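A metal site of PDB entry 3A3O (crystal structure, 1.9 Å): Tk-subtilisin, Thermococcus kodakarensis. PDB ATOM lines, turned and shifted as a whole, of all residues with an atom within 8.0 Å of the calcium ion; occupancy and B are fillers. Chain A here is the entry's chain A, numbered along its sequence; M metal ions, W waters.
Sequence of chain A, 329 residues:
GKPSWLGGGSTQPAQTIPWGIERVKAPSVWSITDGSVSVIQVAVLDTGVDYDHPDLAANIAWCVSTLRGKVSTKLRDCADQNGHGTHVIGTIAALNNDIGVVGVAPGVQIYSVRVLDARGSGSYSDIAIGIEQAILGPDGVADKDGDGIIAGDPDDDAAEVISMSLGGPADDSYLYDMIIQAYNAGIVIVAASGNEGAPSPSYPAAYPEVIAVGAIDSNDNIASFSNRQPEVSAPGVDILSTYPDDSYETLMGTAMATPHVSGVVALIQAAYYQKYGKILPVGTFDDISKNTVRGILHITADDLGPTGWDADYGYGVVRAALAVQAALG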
ATOM      1  N   VAL A  37      19.781  -8.369 -31.012  1.00  0.00           N
ATOM      2  CA  VAL A  37      18.933  -8.454 -29.827  1.00  0.00           C
ATOM      3  C   VAL A  37      19.836  -9.066 -28.725  1.00  0.00           C
ATOM      4  O   VAL A  37      20.456 -10.122 -28.946  1.00  0.00           O
ATOM      5  CB  VAL A  37      17.673  -9.323 -30.160  1.00  0.00           C
ATOM      6  CG1 VAL A  37      16.882  -9.703 -28.907  1.00  0.00           C
ATOM      7  CG2 VAL A  37      16.770  -8.582 -31.171  1.00  0.00           C
ATOM      8  N   SER A  38      19.963  -8.399 -27.565  1.00  0.00           N
ATOM      9  CA  SER A  38      21.059  -8.738 -26.640  1.00  0.00           C
ATOM     10  C   SER A  38      21.086 -10.172 -26.062  1.00  0.00           C
ATOM     11  O   SER A  38      22.156 -10.673 -25.696  1.00  0.00           O
ATOM     12  CB  SER A  38      21.170  -7.701 -25.501  1.00  0.00           C
ATOM     13  OG  SER A  38      20.060  -7.787 -24.618  1.00  0.00           O
ATOM     14  N   VAL A  39      19.937 -10.814 -25.985  1.00  0.00           N
ATOM     15  CA  VAL A  39      19.898 -12.190 -25.432  1.00  0.00           C
ATOM     16  C   VAL A  39      20.371 -13.250 -26.452  1.00  0.00           C
ATOM     17  O   VAL A  39      20.669 -14.395 -26.071  1.00  0.00           O
ATOM     18  CB  VAL A  39      18.459 -12.588 -24.972  1.00  0.00           C
ATOM     19  CG1 VAL A  39      17.548 -12.797 -26.183  1.00  0.00           C
ATOM     20  CG2 VAL A  39      18.480 -13.891 -24.127  1.00  0.00           C
ATOM     21  N   ILE A  40      20.452 -12.853 -27.734  1.00  0.00           N
ATOM     22  CA  ILE A  40      20.769 -13.809 -28.822  1.00  0.00           C
ATOM     23  C   ILE A  40      22.283 -13.877 -29.105  1.00  0.00           C
ATOM     24  O   ILE A  40      22.897 -12.852 -29.398  1.00  0.00           O
ATOM     25  CB  ILE A  40      20.041 -13.436 -30.152  1.00  0.00           C
ATOM     26  CG1 ILE A  40      18.517 -13.369 -29.965  1.00  0.00           C
ATOM     27  CG2 ILE A  40      20.472 -14.400 -31.334  1.00  0.00           C
ATOM     28  CD1 ILE A  40      17.872 -14.702 -29.525  1.00  0.00           C
ATOM     29  N   GLN A  41      22.869 -15.068 -29.001  1.00  0.00           N
ATOM     30  CA  GLN A  41      24.240 -15.304 -29.522  1.00  0.00           C
ATOM     31  C   GLN A  41      24.275 -16.556 -30.406  1.00  0.00           C
ATOM     32  O   GLN A  41      23.516 -17.498 -30.189  1.00  0.00           O
ATOM     33  CB  GLN A  41      25.260 -15.508 -28.391  1.00  0.00           C
ATOM     34  CG  GLN A  41      25.372 -14.370 -27.381  1.00  0.00           C
ATOM     35  CD  GLN A  41      24.245 -14.317 -26.347  1.00  0.00           C
ATOM     36  OE1 GLN A  41      23.653 -15.342 -25.944  1.00  0.00           O
ATOM     37  NE2 GLN A  41      23.981 -13.123 -25.863  1.00  0.00           N
ATOM     38  N   VAL A  42      25.184 -16.570 -31.393  1.00  0.00           N
ATOM     39  CA  VAL A  42      25.363 -17.748 -32.232  1.00  0.00           C
ATOM     40  C   VAL A  42      26.753 -18.307 -31.937  1.00  0.00           C
ATOM     41  O   VAL A  42      27.740 -17.591 -32.064  1.00  0.00           O
ATOM     42  CB  VAL A  42      25.245 -17.428 -33.730  1.00  0.00           C
ATOM     43  CG1 VAL A  42      25.611 -18.677 -34.564  1.00  0.00           C
ATOM     44  CG2 VAL A  42      23.784 -16.921 -34.089  1.00  0.00           C
ATOM     45  N   GLN A 109      25.584 -11.242 -32.126  1.00  0.00           N
ATOM     46  CA  GLN A 109      26.742 -11.616 -31.322  1.00  0.00           C
ATOM     47  C   GLN A 109      27.199 -13.041 -31.643  1.00  0.00           C
ATOM     48  O   GLN A 109      26.374 -13.963 -31.724  1.00  0.00           O
ATOM     49  CB  GLN A 109      26.379 -11.572 -29.839  1.00  0.00           C
ATOM     50  CG  GLN A 109      26.041 -10.189 -29.311  1.00  0.00           C
ATOM     51  CD  GLN A 109      25.538 -10.248 -27.884  1.00  0.00           C
ATOM     52  OE1 GLN A 109      26.033 -11.025 -27.071  1.00  0.00           O
ATOM     53  NE2 GLN A 109      24.528  -9.446 -27.569  1.00  0.00           N
ATOM     54  N   TYR A 111      29.777 -16.250 -30.520  1.00  0.00           N
ATOM     55  CA  TYR A 111      30.762 -16.956 -29.723  1.00  0.00           C
ATOM     56  C   TYR A 111      31.606 -17.801 -30.668  1.00  0.00           C
ATOM     57  O   TYR A 111      31.105 -18.759 -31.286  1.00  0.00           O
ATOM     58  CB  TYR A 111      30.065 -17.907 -28.720  1.00  0.00           C
ATOM     59  CG  TYR A 111      29.248 -17.271 -27.625  1.00  0.00           C
ATOM     60  CD1 TYR A 111      29.349 -15.903 -27.309  1.00  0.00           C
ATOM     61  CD2 TYR A 111      28.432 -18.067 -26.822  1.00  0.00           C
ATOM     62  CE1 TYR A 111      28.630 -15.348 -26.255  1.00  0.00           C
ATOM     63  CE2 TYR A 111      27.715 -17.507 -25.746  1.00  0.00           C
ATOM     64  CZ  TYR A 111      27.816 -16.164 -25.484  1.00  0.00           C
ATOM     65  OH  TYR A 111      27.096 -15.652 -24.432  1.00  0.00           O
ATOM     66  N   ALA A 134      29.345 -23.816 -25.421  1.00  0.00           N
ATOM     67  CA  ALA A 134      28.258 -22.997 -26.000  1.00  0.00           C
ATOM     68  C   ALA A 134      27.029 -22.942 -25.098  1.00  0.00           C
ATOM     69  O   ALA A 134      26.269 -21.955 -25.118  1.00  0.00           O
ATOM     70  CB  ALA A 134      27.853 -23.528 -27.394  1.00  0.00           C
ATOM     71  N   ILE A 150      17.209 -21.855 -20.700  1.00  0.00           N
ATOM     72  CA  ILE A 150      18.640 -21.649 -20.956  1.00  0.00           C
ATOM     73  C   ILE A 150      18.802 -20.765 -22.204  1.00  0.00           C
ATOM     74  O   ILE A 150      19.079 -19.570 -22.060  1.00  0.00           O
ATOM     75  CB  ILE A 150      19.430 -23.013 -21.015  1.00  0.00           C
ATOM     76  CG1 ILE A 150      19.306 -23.774 -19.686  1.00  0.00           C
ATOM     77  CG2 ILE A 150      20.931 -22.744 -21.363  1.00  0.00           C
ATOM     78  CD1 ILE A 150      19.790 -25.235 -19.680  1.00  0.00           C
ATOM     79  N   ALA A 151      18.629 -21.330 -23.402  1.00  0.00           N
ATOM     80  CA  ALA A 151      18.490 -20.485 -24.601  1.00  0.00           C
ATOM     81  C   ALA A 151      17.313 -19.528 -24.384  1.00  0.00           C
ATOM     82  O   ALA A 151      16.265 -19.955 -23.911  1.00  0.00           O
ATOM     83  CB  ALA A 151      18.275 -21.329 -25.880  1.00  0.00           C
ATOM     84  N   GLY A 152      17.504 -18.258 -24.726  1.00  0.00           N
ATOM     85  CA  GLY A 152      16.448 -17.253 -24.576  1.00  0.00           C
ATOM     86  C   GLY A 152      16.192 -16.680 -23.175  1.00  0.00           C
ATOM     87  O   GLY A 152      15.350 -15.781 -23.036  1.00  0.00           O
ATOM     88  N   ASP A 153      16.885 -17.174 -22.154  1.00  0.00           N
ATOM     89  CA  ASP A 153      16.768 -16.604 -20.807  1.00  0.00           C
ATOM     90  C   ASP A 153      17.747 -15.452 -20.659  1.00  0.00           C
ATOM     91  O   ASP A 153      18.963 -15.676 -20.722  1.00  0.00           O
ATOM     92  CB  ASP A 153      17.017 -17.655 -19.706  1.00  0.00           C
ATOM     93  CG  ASP A 153      16.751 -17.117 -18.299  1.00  0.00           C
ATOM     94  OD1 ASP A 153      16.577 -17.917 -17.350  1.00  0.00           O
ATOM     95  OD2 ASP A 153      16.742 -15.867 -18.126  1.00  0.00           O
ATOM     96  N   PRO A 154      17.234 -14.217 -20.469  1.00  0.00           N
ATOM     97  CA  PRO A 154      18.181 -13.093 -20.445  1.00  0.00           C
ATOM     98  C   PRO A 154      19.120 -13.104 -19.220  1.00  0.00           C
ATOM     99  O   PRO A 154      20.163 -12.439 -19.232  1.00  0.00           O
ATOM    100  CB  PRO A 154      17.263 -11.851 -20.461  1.00  0.00           C
ATOM    101  CG  PRO A 154      15.931 -12.388 -19.814  1.00  0.00           C
ATOM    102  CD  PRO A 154      15.837 -13.800 -20.318  1.00  0.00           C
ATOM    103  N   ASP A 155      18.742 -13.860 -18.189  1.00  0.00           N
ATOM    104  CA  ASP A 155      19.607 -14.093 -17.031  1.00  0.00           C
ATOM    105  C   ASP A 155      20.786 -15.024 -17.328  1.00  0.00           C
ATOM    106  O   ASP A 155      21.773 -15.003 -16.597  1.00  0.00           O
ATOM    107  CB  ASP A 155      18.803 -14.619 -15.822  1.00  0.00           C
ATOM    108  CG  ASP A 155      19.626 -14.620 -14.545  1.00  0.00           C
ATOM    109  OD1 ASP A 155      20.141 -13.541 -14.155  1.00  0.00           O
ATOM    110  OD2 ASP A 155      19.795 -15.708 -13.956  1.00  0.00           O
ATOM    111  N   ASP A 156      20.698 -15.841 -18.373  1.00  0.00           N
ATOM    112  CA  ASP A 156      21.804 -16.731 -18.750  1.00  0.00           C
ATOM    113  C   ASP A 156      22.529 -16.217 -19.992  1.00  0.00           C
ATOM    114  O   ASP A 156      22.039 -15.314 -20.681  1.00  0.00           O
ATOM    115  CB  ASP A 156      21.284 -18.147 -18.987  1.00  0.00           C
ATOM    116  CG  ASP A 156      20.944 -18.870 -17.694  1.00  0.00           C
ATOM    117  OD1 ASP A 156      21.870 -19.040 -16.857  1.00  0.00           O
ATOM    118  OD2 ASP A 156      19.761 -19.276 -17.528  1.00  0.00           O
ATOM    119  N   ASP A 157      23.672 -16.836 -20.300  1.00  0.00           N
ATOM    120  CA  ASP A 157      24.507 -16.374 -21.411  1.00  0.00           C
ATOM    121  C   ASP A 157      24.762 -17.489 -22.443  1.00  0.00           C
ATOM    122  O   ASP A 157      25.732 -17.431 -23.222  1.00  0.00           O
ATOM    123  CB  ASP A 157      25.852 -15.852 -20.849  1.00  0.00           C
ATOM    124  CG  ASP A 157      26.590 -16.894 -20.007  1.00  0.00           C
ATOM    125  OD1 ASP A 157      27.659 -16.536 -19.440  1.00  0.00           O
ATOM    126  OD2 ASP A 157      26.143 -18.086 -19.877  1.00  0.00           O
ATOM    127  N   ALA A 158      23.889 -18.486 -22.459  1.00  0.00           N
ATOM    128  CA  ALA A 158      23.998 -19.571 -23.415  1.00  0.00           C
ATOM    129  C   ALA A 158      23.722 -19.037 -24.828  1.00  0.00           C
ATOM    130  O   ALA A 158      22.942 -18.112 -24.993  1.00  0.00           O
ATOM    131  CB  ALA A 158      22.970 -20.648 -23.084  1.00  0.00           C
ATOM    132  N   ALA A 159      24.333 -19.681 -25.814  1.00  0.00           N
ATOM    133  CA  ALA A 159      24.011 -19.453 -27.219  1.00  0.00           C
ATOM    134  C   ALA A 159      22.612 -19.996 -27.557  1.00  0.00           C
ATOM    135  O   ALA A 159      22.121 -20.932 -26.902  1.00  0.00           O
ATOM    136  CB  ALA A 159      25.069 -20.145 -28.126  1.00  0.00           C
ATOM    137  N   GLU A 160      22.008 -19.437 -28.602  1.00  0.00           N
ATOM    138  CA  GLU A 160      20.674 -19.831 -29.059  1.00  0.00           C
ATOM    139  C   GLU A 160      20.777 -20.675 -30.323  1.00  0.00           C
ATOM    140  O   GLU A 160      19.809 -21.350 -30.718  1.00  0.00           O
ATOM    141  CB  GLU A 160      19.800 -18.599 -29.343  1.00  0.00           C
ATOM    142  CG  GLU A 160      19.115 -18.015 -28.090  1.00  0.00           C
ATOM    143  CD  GLU A 160      20.089 -17.430 -27.107  1.00  0.00           C
ATOM    144  OE1 GLU A 160      19.787 -17.438 -25.902  1.00  0.00           O
ATOM    145  OE2 GLU A 160      21.178 -16.936 -27.512  1.00  0.00           O
ATOM    146  N   VAL A 161      21.940 -20.619 -30.975  1.00  0.00           N
ATOM    147  CA  VAL A 161      22.238 -21.382 -32.191  1.00  0.00           C
ATOM    148  C   VAL A 161      23.625 -21.955 -32.022  1.00  0.00           C
ATOM    149  O   VAL A 161      24.555 -21.240 -31.594  1.00  0.00           O
ATOM    150  CB  VAL A 161      22.211 -20.523 -33.503  1.00  0.00           C
ATOM    151  CG1 VAL A 161      22.316 -21.418 -34.749  1.00  0.00           C
ATOM    152  CG2 VAL A 161      20.962 -19.651 -33.593  1.00  0.00           C
ATOM    153  N   ILE A 187      18.377 -24.891 -27.729  1.00  0.00           N
ATOM    154  CA  ILE A 187      19.326 -24.386 -28.744  1.00  0.00           C
ATOM    155  C   ILE A 187      19.059 -25.083 -30.090  1.00  0.00           C
ATOM    156  O   ILE A 187      18.912 -26.333 -30.151  1.00  0.00           O
ATOM    157  CB  ILE A 187      20.789 -24.609 -28.292  1.00  0.00           C
ATOM    158  CG1 ILE A 187      21.022 -23.904 -26.955  1.00  0.00           C
ATOM    159  CG2 ILE A 187      21.807 -24.078 -29.369  1.00  0.00           C
ATOM    160  CD1 ILE A 187      22.386 -24.298 -26.261  1.00  0.00           C
ATOM    161  N   ILE A 279      11.669 -16.974 -27.104  1.00  0.00           N
ATOM    162  CA  ILE A 279      12.130 -17.550 -28.366  1.00  0.00           C
ATOM    163  C   ILE A 279      11.201 -18.686 -28.749  1.00  0.00           C
ATOM    164  O   ILE A 279      10.409 -19.108 -27.925  1.00  0.00           O
ATOM    165  CB  ILE A 279      13.636 -18.003 -28.302  1.00  0.00           C
ATOM    166  CG1 ILE A 279      13.870 -19.073 -27.227  1.00  0.00           C
ATOM    167  CG2 ILE A 279      14.536 -16.768 -28.128  1.00  0.00           C
ATOM    168  CD1 ILE A 279      15.226 -19.795 -27.379  1.00  0.00           C
HETATM  169 CA    CA M   1      21.707 -16.176 -25.195  1.00  0.00          CA
HETATM  170  O   HOH W   1      22.019 -14.562 -23.360  1.00  0.00           O
HETATM  171  O   HOH W   2      20.494 -17.096 -22.951  1.00  0.00           O
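Water W1 lies within hydrogen-bond range of the backbone carbonyl oxygen of Asp 156 (2.8 Å) and the side-chain amide nitrogen of Gln 41 (3.5 Å).
O of Ser 38 sits at hydrogen-bond distance from NE2 of Gln 41. The side-chain amide nitrogen (NE2) of Gln 41 sits at hydrogen-bond distance from the side-chain amide oxygen (OE1) of Gln 109 (3.2 Å). N of Gly 152 sits close to OE1 of Glu 160 (2.7 Å).
Within 4 Å of the calcium ion: Val 39, Gln 41, Ala 158 and Glu 160.
The calcium ion is bound by the backbone carbonyl oxygen (O) of Val 39, the side-chain amide oxygen (OE1) of Gln 41, the backbone carbonyl oxygen (O) of Ala 158, the side-chain carboxylate (OE1) of Glu 160, water W1, the side-chain carboxylate (OE2) of Glu 160 and water W2.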
